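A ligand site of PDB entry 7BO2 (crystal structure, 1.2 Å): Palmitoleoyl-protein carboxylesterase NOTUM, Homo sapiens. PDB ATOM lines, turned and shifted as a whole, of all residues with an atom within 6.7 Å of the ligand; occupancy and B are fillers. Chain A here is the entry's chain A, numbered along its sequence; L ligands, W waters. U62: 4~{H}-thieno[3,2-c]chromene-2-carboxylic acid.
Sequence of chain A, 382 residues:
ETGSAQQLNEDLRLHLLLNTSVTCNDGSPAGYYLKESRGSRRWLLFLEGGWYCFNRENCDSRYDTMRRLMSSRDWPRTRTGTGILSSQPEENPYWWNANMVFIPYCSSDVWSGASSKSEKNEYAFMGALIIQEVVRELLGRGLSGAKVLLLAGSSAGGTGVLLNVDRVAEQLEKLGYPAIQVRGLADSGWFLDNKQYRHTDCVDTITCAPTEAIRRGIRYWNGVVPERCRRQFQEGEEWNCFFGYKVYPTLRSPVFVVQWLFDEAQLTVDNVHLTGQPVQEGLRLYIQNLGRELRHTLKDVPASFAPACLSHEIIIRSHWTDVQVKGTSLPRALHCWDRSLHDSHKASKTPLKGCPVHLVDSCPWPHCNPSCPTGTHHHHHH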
ATOM      1  N   GLY A  49     -27.615   2.922  -5.084  1.00  0.00           N
ATOM      2  CA  GLY A  49     -26.865   1.697  -5.217  1.00  0.00           C
ATOM      3  C   GLY A  49     -26.550   1.313  -6.662  1.00  0.00           C
ATOM      4  O   GLY A  49     -26.698   2.108  -7.589  1.00  0.00           O
ATOM      5  N   GLY A  50     -26.099   0.059  -6.833  1.00  0.00           N
ATOM      6  CA  GLY A  50     -25.734  -0.459  -8.151  1.00  0.00           C
ATOM      7  C   GLY A  50     -24.438  -1.255  -8.283  1.00  0.00           C
ATOM      8  O   GLY A  50     -23.642  -1.020  -9.204  1.00  0.00           O
ATOM      9  N   TRP A  51     -24.232  -2.208  -7.382  1.00  0.00           N
ATOM     10  CA  TRP A  51     -23.082  -3.139  -7.390  1.00  0.00           C
ATOM     11  C   TRP A  51     -21.782  -2.331  -7.225  1.00  0.00           C
ATOM     12  O   TRP A  51     -21.771  -1.385  -6.413  1.00  0.00           O
ATOM     13  CB  TRP A  51     -23.136  -4.148  -8.551  1.00  0.00           C
ATOM     14  CG  TRP A  51     -24.334  -5.079  -8.470  1.00  0.00           C
ATOM     15  CD1 TRP A  51     -25.577  -4.857  -8.991  1.00  0.00           C
ATOM     16  CD2 TRP A  51     -24.395  -6.359  -7.831  1.00  0.00           C
ATOM     17  NE1 TRP A  51     -26.403  -5.924  -8.712  1.00  0.00           N
ATOM     18  CE2 TRP A  51     -25.706  -6.860  -8.005  1.00  0.00           C
ATOM     19  CE3 TRP A  51     -23.465  -7.139  -7.125  1.00  0.00           C
ATOM     20  CZ2 TRP A  51     -26.102  -8.092  -7.513  1.00  0.00           C
ATOM     21  CZ3 TRP A  51     -23.869  -8.370  -6.638  1.00  0.00           C
ATOM     22  CH2 TRP A  51     -25.178  -8.830  -6.824  1.00  0.00           C
ATOM     23  N   TYR A  52     -20.711  -2.695  -7.924  1.00  0.00           N
ATOM     24  CA  TYR A  52     -19.367  -2.139  -7.750  1.00  0.00           C
ATOM     25  C   TYR A  52     -18.466  -2.771  -8.818  1.00  0.00           C
ATOM     26  O   TYR A  52     -18.898  -3.674  -9.536  1.00  0.00           O
ATOM     27  CB  TYR A  52     -18.817  -2.376  -6.338  1.00  0.00           C
ATOM     28  CG  TYR A  52     -18.778  -3.820  -5.854  1.00  0.00           C
ATOM     29  CD1 TYR A  52     -17.631  -4.590  -6.016  1.00  0.00           C
ATOM     30  CD2 TYR A  52     -19.865  -4.373  -5.162  1.00  0.00           C
ATOM     31  CE1 TYR A  52     -17.574  -5.887  -5.545  1.00  0.00           C
ATOM     32  CE2 TYR A  52     -19.815  -5.682  -4.701  1.00  0.00           C
ATOM     33  CZ  TYR A  52     -18.655  -6.433  -4.894  1.00  0.00           C
ATOM     34  OH  TYR A  52     -18.577  -7.732  -4.435  1.00  0.00           O
ATOM     35  N   TYR A 105     -24.672   7.530  -7.303  1.00  0.00           N
ATOM     36  CA  TYR A 105     -23.564   6.595  -7.082  1.00  0.00           C
ATOM     37  C   TYR A 105     -22.715   6.582  -8.350  1.00  0.00           C
ATOM     38  O   TYR A 105     -23.099   6.011  -9.361  1.00  0.00           O
ATOM     39  CB  TYR A 105     -24.145   5.218  -6.791  1.00  0.00           C
ATOM     40  CG  TYR A 105     -23.185   4.082  -6.474  1.00  0.00           C
ATOM     41  CD1 TYR A 105     -22.054   4.281  -5.696  1.00  0.00           C
ATOM     42  CD2 TYR A 105     -23.457   2.779  -6.926  1.00  0.00           C
ATOM     43  CE1 TYR A 105     -21.205   3.211  -5.383  1.00  0.00           C
ATOM     44  CE2 TYR A 105     -22.621   1.715  -6.612  1.00  0.00           C
ATOM     45  CZ  TYR A 105     -21.502   1.925  -5.848  1.00  0.00           C
ATOM     46  OH  TYR A 105     -20.671   0.866  -5.526  1.00  0.00           O
ATOM     47  N   VAL A 110     -18.852   0.903  -3.255  1.00  0.00           N
ATOM     48  CA  VAL A 110     -19.739   0.723  -2.093  1.00  0.00           C
ATOM     49  C   VAL A 110     -19.597   1.918  -1.137  1.00  0.00           C
ATOM     50  O   VAL A 110     -19.777   1.782   0.085  1.00  0.00           O
ATOM     51  CB  VAL A 110     -19.529  -0.646  -1.400  1.00  0.00           C
ATOM     52  CG1 VAL A 110     -20.782  -1.023  -0.562  1.00  0.00           C
ATOM     53  CG2 VAL A 110     -19.238  -1.744  -2.422  1.00  0.00           C
ATOM     54  N   SER A 154     -30.113   2.572  -0.598  1.00  0.00           N
ATOM     55  CA  SER A 154     -30.564   1.257  -1.062  1.00  0.00           C
ATOM     56  C   SER A 154     -29.425   0.479  -1.731  1.00  0.00           C
ATOM     57  O   SER A 154     -28.614   1.059  -2.467  1.00  0.00           O
ATOM     58  CB  SER A 154     -31.742   1.358  -2.041  1.00  0.00           C
ATOM     59  OG  SER A 154     -32.890   1.959  -1.430  1.00  0.00           O
ATOM     60  N   SER A 155     -29.398  -0.846  -1.501  1.00  0.00           N
ATOM     61  CA  SER A 155     -28.418  -1.768  -2.115  1.00  0.00           C
ATOM     62  C   SER A 155     -27.007  -1.358  -1.702  1.00  0.00           C
ATOM     63  O   SER A 155     -26.744  -1.221  -0.488  1.00  0.00           O
ATOM     64  CB  SER A 155     -28.675  -1.876  -3.624  1.00  0.00           C
ATOM     65  OG  SER A 155     -30.031  -2.193  -3.872  1.00  0.00           O
ATOM     66  N   ALA A 156     -26.069  -1.151  -2.636  1.00  0.00           N
ATOM     67  CA  ALA A 156     -24.750  -0.644  -2.247  1.00  0.00           C
ATOM     68  C   ALA A 156     -24.848   0.646  -1.421  1.00  0.00           C
ATOM     69  O   ALA A 156     -23.987   0.901  -0.568  1.00  0.00           O
ATOM     70  CB  ALA A 156     -23.847  -0.426  -3.475  1.00  0.00           C
ATOM     71  N   GLY A 157     -25.877   1.470  -1.671  1.00  0.00           N
ATOM     72  CA  GLY A 157     -26.107   2.657  -0.838  1.00  0.00           C
ATOM     73  C   GLY A 157     -26.522   2.336   0.588  1.00  0.00           C
ATOM     74  O   GLY A 157     -26.190   3.094   1.519  1.00  0.00           O
ATOM     75  N   THR A 159     -25.465  -0.422   2.255  1.00  0.00           N
ATOM     76  CA  THR A 159     -24.173  -0.735   2.862  1.00  0.00           C
ATOM     77  C   THR A 159     -23.380   0.550   3.121  1.00  0.00           C
ATOM     78  O   THR A 159     -22.731   0.690   4.177  1.00  0.00           O
ATOM     79  CB  THR A 159     -23.372  -1.714   1.984  1.00  0.00           C
ATOM     80  OG1 THR A 159     -24.202  -2.806   1.556  1.00  0.00           O
ATOM     81  CG2 THR A 159     -22.152  -2.230   2.737  1.00  0.00           C
ATOM     82  N   SER A 188     -31.755  -2.901   2.001  1.00  0.00           N
ATOM     83  CA  SER A 188     -31.232  -3.906   1.055  1.00  0.00           C
ATOM     84  C   SER A 188     -29.705  -3.891   0.971  1.00  0.00           C
ATOM     85  O   SER A 188     -29.107  -4.213  -0.079  1.00  0.00           O
ATOM     86  CB  SER A 188     -31.881  -3.777  -0.326  1.00  0.00           C
ATOM     87  OG  SER A 188     -33.296  -3.917  -0.215  1.00  0.00           O
ATOM     88  N   GLY A 189     -29.039  -3.570   2.074  1.00  0.00           N
ATOM     89  CA  GLY A 189     -27.593  -3.586   2.131  1.00  0.00           C
ATOM     90  C   GLY A 189     -27.002  -4.468   3.218  1.00  0.00           C
ATOM     91  O   GLY A 189     -25.828  -4.291   3.571  1.00  0.00           O
ATOM     92  N   PHE A 191     -25.997  -8.075   4.013  1.00  0.00           N
ATOM     93  CA  PHE A 191     -25.659  -9.308   3.331  1.00  0.00           C
ATOM     94  C   PHE A 191     -24.947 -10.288   4.248  1.00  0.00           C
ATOM     95  O   PHE A 191     -24.343  -9.906   5.261  1.00  0.00           O
ATOM     96  CB  PHE A 191     -24.833  -9.026   2.067  1.00  0.00           C
ATOM     97  CG  PHE A 191     -25.560  -8.175   1.059  1.00  0.00           C
ATOM     98  CD1 PHE A 191     -25.234  -6.834   0.857  1.00  0.00           C
ATOM     99  CD2 PHE A 191     -26.636  -8.709   0.361  1.00  0.00           C
ATOM    100  CE1 PHE A 191     -25.939  -6.049  -0.057  1.00  0.00           C
ATOM    101  CE2 PHE A 191     -27.341  -7.929  -0.536  1.00  0.00           C
ATOM    102  CZ  PHE A 191     -26.989  -6.599  -0.742  1.00  0.00           C
ATOM    103  N   LEU A 192     -25.006 -11.578   3.882  1.00  0.00           N
ATOM    104  CA  LEU A 192     -24.357 -12.658   4.608  1.00  0.00           C
ATOM    105  C   LEU A 192     -23.176 -13.217   3.804  1.00  0.00           C
ATOM    106  O   LEU A 192     -23.291 -13.465   2.604  1.00  0.00           O
ATOM    107  CB  LEU A 192     -25.347 -13.785   4.914  1.00  0.00           C
ATOM    108  CG  LEU A 192     -26.608 -13.456   5.714  1.00  0.00           C
ATOM    109  CD1 LEU A 192     -27.446 -14.708   5.939  1.00  0.00           C
ATOM    110  CD2 LEU A 192     -26.255 -12.785   7.030  1.00  0.00           C
ATOM    111  N   PRO A 210     -18.367 -12.687  -2.875  1.00  0.00           N
ATOM    112  CA  PRO A 210     -18.293 -11.315  -2.324  1.00  0.00           C
ATOM    113  C   PRO A 210     -17.124 -11.042  -1.394  1.00  0.00           C
ATOM    114  O   PRO A 210     -16.511  -9.968  -1.479  1.00  0.00           O
ATOM    115  CB  PRO A 210     -19.643 -11.161  -1.606  1.00  0.00           C
ATOM    116  CG  PRO A 210     -20.549 -12.077  -2.323  1.00  0.00           C
ATOM    117  CD  PRO A 210     -19.717 -13.258  -2.751  1.00  0.00           C
ATOM    118  N   THR A 211     -16.792 -11.977  -0.492  1.00  0.00           N
ATOM    119  CA  THR A 211     -15.675 -11.725   0.419  1.00  0.00           C
ATOM    120  C   THR A 211     -14.370 -11.515  -0.351  1.00  0.00           C
ATOM    121  O   THR A 211     -13.578 -10.640  -0.001  1.00  0.00           O
ATOM    122  CB  THR A 211     -15.534 -12.844   1.447  1.00  0.00           C
ATOM    123  OG1 THR A 211     -15.326 -14.091   0.771  1.00  0.00           O
ATOM    124  CG2 THR A 211     -16.778 -12.935   2.330  1.00  0.00           C
ATOM    125  N   ILE A 214     -14.591  -8.118  -2.467  1.00  0.00           N
ATOM    126  CA  ILE A 214     -14.453  -6.936  -1.612  1.00  0.00           C
ATOM    127  C   ILE A 214     -13.028  -6.813  -1.068  1.00  0.00           C
ATOM    128  O   ILE A 214     -12.491  -5.700  -0.971  1.00  0.00           O
ATOM    129  CB  ILE A 214     -15.516  -6.937  -0.498  1.00  0.00           C
ATOM    130  CG1 ILE A 214     -16.895  -6.695  -1.118  1.00  0.00           C
ATOM    131  CG2 ILE A 214     -15.220  -5.881   0.560  1.00  0.00           C
ATOM    132  CD1 ILE A 214     -18.014  -7.010  -0.179  1.00  0.00           C
ATOM    133  N   PHE A 242     -17.850  -4.725   5.704  1.00  0.00           N
ATOM    134  CA  PHE A 242     -18.855  -4.563   4.651  1.00  0.00           C
ATOM    135  C   PHE A 242     -20.081  -5.458   4.865  1.00  0.00           C
ATOM    136  O   PHE A 242     -21.033  -5.366   4.087  1.00  0.00           O
ATOM    137  CB  PHE A 242     -18.239  -4.833   3.260  1.00  0.00           C
ATOM    138  CG  PHE A 242     -17.343  -3.711   2.738  1.00  0.00           C
ATOM    139  CD1 PHE A 242     -16.145  -3.407   3.375  1.00  0.00           C
ATOM    140  CD2 PHE A 242     -17.664  -3.007   1.585  1.00  0.00           C
ATOM    141  CE1 PHE A 242     -15.318  -2.396   2.878  1.00  0.00           C
ATOM    142  CE2 PHE A 242     -16.833  -2.006   1.096  1.00  0.00           C
ATOM    143  CZ  PHE A 242     -15.668  -1.709   1.743  1.00  0.00           C
ATOM    144  N   PHE A 243     -20.063  -6.312   5.893  1.00  0.00           N
ATOM    145  CA  PHE A 243     -21.160  -7.226   6.200  1.00  0.00           C
ATOM    146  C   PHE A 243     -21.911  -6.703   7.417  1.00  0.00           C
ATOM    147  O   PHE A 243     -21.343  -6.583   8.514  1.00  0.00           O
ATOM    148  CB  PHE A 243     -20.632  -8.662   6.335  1.00  0.00           C
ATOM    149  CG  PHE A 243     -20.166  -9.213   5.008  1.00  0.00           C
ATOM    150  CD1 PHE A 243     -18.872  -8.978   4.549  1.00  0.00           C
ATOM    151  CD2 PHE A 243     -21.049  -9.885   4.170  1.00  0.00           C
ATOM    152  CE1 PHE A 243     -18.462  -9.413   3.290  1.00  0.00           C
ATOM    153  CE2 PHE A 243     -20.636 -10.317   2.924  1.00  0.00           C
ATOM    154  CZ  PHE A 243     -19.350 -10.092   2.492  1.00  0.00           C
ATOM    155  N   ASP A 263     -33.427 -11.766  -0.294  1.00  0.00           N
ATOM    156  CA  ASP A 263     -33.035 -10.709  -1.214  1.00  0.00           C
ATOM    157  C   ASP A 263     -32.448 -11.296  -2.508  1.00  0.00           C
ATOM    158  O   ASP A 263     -31.606 -12.193  -2.479  1.00  0.00           O
ATOM    159  CB  ASP A 263     -32.012  -9.829  -0.495  1.00  0.00           C
ATOM    160  CG  ASP A 263     -31.591  -8.654  -1.309  1.00  0.00           C
ATOM    161  OD1 ASP A 263     -32.250  -7.595  -1.216  1.00  0.00           O
ATOM    162  OD2 ASP A 263     -30.589  -8.798  -2.040  1.00  0.00           O
ATOM    163  N   ALA A 265     -30.316 -10.092  -4.644  1.00  0.00           N
ATOM    164  CA  ALA A 265     -28.858  -9.961  -4.764  1.00  0.00           C
ATOM    165  C   ALA A 265     -28.121 -10.977  -3.889  1.00  0.00           C
ATOM    166  O   ALA A 265     -27.073 -11.512  -4.298  1.00  0.00           O
ATOM    167  CB  ALA A 265     -28.428  -8.528  -4.438  1.00  0.00           C
ATOM    168  N   GLN A 266     -28.641 -11.270  -2.691  1.00  0.00           N
ATOM    169  CA  GLN A 266     -28.090 -12.341  -1.861  1.00  0.00           C
ATOM    170  C   GLN A 266     -28.156 -13.672  -2.605  1.00  0.00           C
ATOM    171  O   GLN A 266     -27.171 -14.423  -2.641  1.00  0.00           O
ATOM    172  CB  GLN A 266     -28.836 -12.428  -0.533  1.00  0.00           C
ATOM    173  CG  GLN A 266     -28.314 -13.516   0.437  1.00  0.00           C
ATOM    174  CD  GLN A 266     -26.982 -13.147   1.092  1.00  0.00           C
ATOM    175  OE1 GLN A 266     -26.863 -12.076   1.709  1.00  0.00           O
ATOM    176  NE2 GLN A 266     -25.988 -14.030   0.982  1.00  0.00           N
ATOM    177  N   VAL A 269     -25.438 -13.826  -5.430  1.00  0.00           N
ATOM    178  CA  VAL A 269     -24.071 -14.085  -4.967  1.00  0.00           C
ATOM    179  C   VAL A 269     -23.939 -15.503  -4.401  1.00  0.00           C
ATOM    180  O   VAL A 269     -22.815 -16.031  -4.327  1.00  0.00           O
ATOM    181  CB  VAL A 269     -23.527 -13.000  -4.024  1.00  0.00           C
ATOM    182  CG1 VAL A 269     -23.570 -11.631  -4.690  1.00  0.00           C
ATOM    183  CG2 VAL A 269     -24.274 -13.000  -2.710  1.00  0.00           C
ATOM    184  N   HIS A 312     -35.900  -6.907  -4.089  1.00  0.00           N
ATOM    185  CA  HIS A 312     -34.658  -6.131  -3.953  1.00  0.00           C
ATOM    186  C   HIS A 312     -34.986  -4.648  -3.924  1.00  0.00           C
ATOM    187  O   HIS A 312     -35.595  -4.141  -4.873  1.00  0.00           O
ATOM    188  CB  HIS A 312     -33.703  -6.458  -5.122  1.00  0.00           C
ATOM    189  CG  HIS A 312     -32.305  -5.922  -4.941  1.00  0.00           C
ATOM    190  ND1 HIS A 312     -31.558  -6.129  -3.796  1.00  0.00           N
ATOM    191  CD2 HIS A 312     -31.513  -5.199  -5.776  1.00  0.00           C
ATOM    192  CE1 HIS A 312     -30.380  -5.552  -3.938  1.00  0.00           C
ATOM    193  NE2 HIS A 312     -30.325  -4.990  -5.127  1.00  0.00           N
ATOM    194  N   GLU A 313     -34.561  -3.948  -2.859  1.00  0.00           N
ATOM    195  CA  GLU A 313     -34.828  -2.520  -2.598  1.00  0.00           C
ATOM    196  C   GLU A 313     -36.280  -2.265  -2.219  1.00  0.00           C
ATOM    197  O   GLU A 313     -37.160  -3.064  -2.551  1.00  0.00           O
ATOM    198  CB  GLU A 313     -34.391  -1.608  -3.747  1.00  0.00           C
ATOM    199  CG  GLU A 313     -32.941  -1.777  -4.140  1.00  0.00           C
ATOM    200  CD  GLU A 313     -32.483  -0.765  -5.177  1.00  0.00           C
ATOM    201  OE1 GLU A 313     -31.323  -0.329  -5.099  1.00  0.00           O
ATOM    202  OE2 GLU A 313     -33.286  -0.425  -6.079  1.00  0.00           O
HETATM  203  C10 U62 L   1     -21.762  -7.938  -0.258  1.00  0.00           C
HETATM  204  C13 U62 L   1     -22.340  -5.237  -0.534  1.00  0.00           C
HETATM  205  C15 U62 L   1     -23.664  -5.734  -2.517  1.00  0.00           C
HETATM  206  C02 U62 L   1     -26.112  -3.867  -5.154  1.00  0.00           C
HETATM  207  C04 U62 L   1     -25.288  -4.749  -4.252  1.00  0.00           C
HETATM  208  C05 U62 L   1     -25.325  -6.129  -4.149  1.00  0.00           C
HETATM  209  C06 U62 L   1     -24.441  -6.652  -3.190  1.00  0.00           C
HETATM  210  C07 U62 L   1     -24.317  -8.155  -2.870  1.00  0.00           C
HETATM  211  C09 U62 L   1     -22.555  -7.491  -1.325  1.00  0.00           C
HETATM  212  C11 U62 L   1     -21.278  -7.035   0.680  1.00  0.00           C
HETATM  213  C12 U62 L   1     -21.561  -5.678   0.535  1.00  0.00           C
HETATM  214  C14 U62 L   1     -22.819  -6.153  -1.500  1.00  0.00           C
HETATM  215  O01 U62 L   1     -25.845  -2.628  -5.172  1.00  0.00           O
HETATM  216  O03 U62 L   1     -27.087  -4.351  -5.792  1.00  0.00           O
HETATM  217  O08 U62 L   1     -23.057  -8.482  -2.274  1.00  0.00           O
HETATM  218  S16 U62 L   1     -24.126  -4.167  -3.130  1.00  0.00           S
HETATM  219  O   HOH W   1     -20.735  -9.105  -3.969  1.00  0.00           O
HETATM  220  O   HOH W   2     -28.642  -2.843  -7.259  1.00  0.00           O
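N of Trp 51 sits at hydrogen-bond distance from O01 of the ligand (2.8 Å). NE1 of Trp 51 lies within hydrogen-bond range of O03 of the ligand, 3.4 Å away. An oxygen (O01) of the ligand lies within hydrogen-bond range of the backbone NH (N) of Ala 156, at 2.9 Å. The backbone NH (N) of Gly 50 sits at hydrogen-bond distance from an oxygen (O01) of the ligand (3.2 Å). O03 of the ligand is in hydrogen-bond range of NE2 of His 312, at 3.4 Å.
OH of Tyr 105 is in hydrogen-bond range of O of Trp 51, 2.7 Å away. The side-chain hydroxyl (OG) of Ser 155 is in hydrogen-bond range of a ring nitrogen (NE2) of His 312, 3.1 Å away. OE1 of Glu 313 is in hydrogen-bond range of OG of Ser 155 (2.6 Å). A ring nitrogen (ND1) of His 312 is in hydrogen-bond range of the side-chain carboxylate of Asp 263 (3.0 Å). The side-chain hydroxyl (OG1) of Thr 159 sits at hydrogen-bond distance from the backbone carbonyl oxygen (O) of Gly 189. The backbone NH of Ala 265 is in hydrogen-bond range of the side-chain carboxylate of Asp 263.
Merely in contact with the ligand: Ser 155 (3.3 Å), Thr 159 (3.7 Å), Phe 191 (3.4 Å), Ile 214 (3.4 Å), Phe 242 (3.6 Å), Ala 265 (3.9 Å) and Val 269 (3.99 Å). The nearest printed residue that does not touch the ligand is Phe 243 (4.03 Å).
Water W2 bridges O03 of the ligand and NE2 of His 312. Water W1 bridges OH of Tyr 52 and O08 of the ligand.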
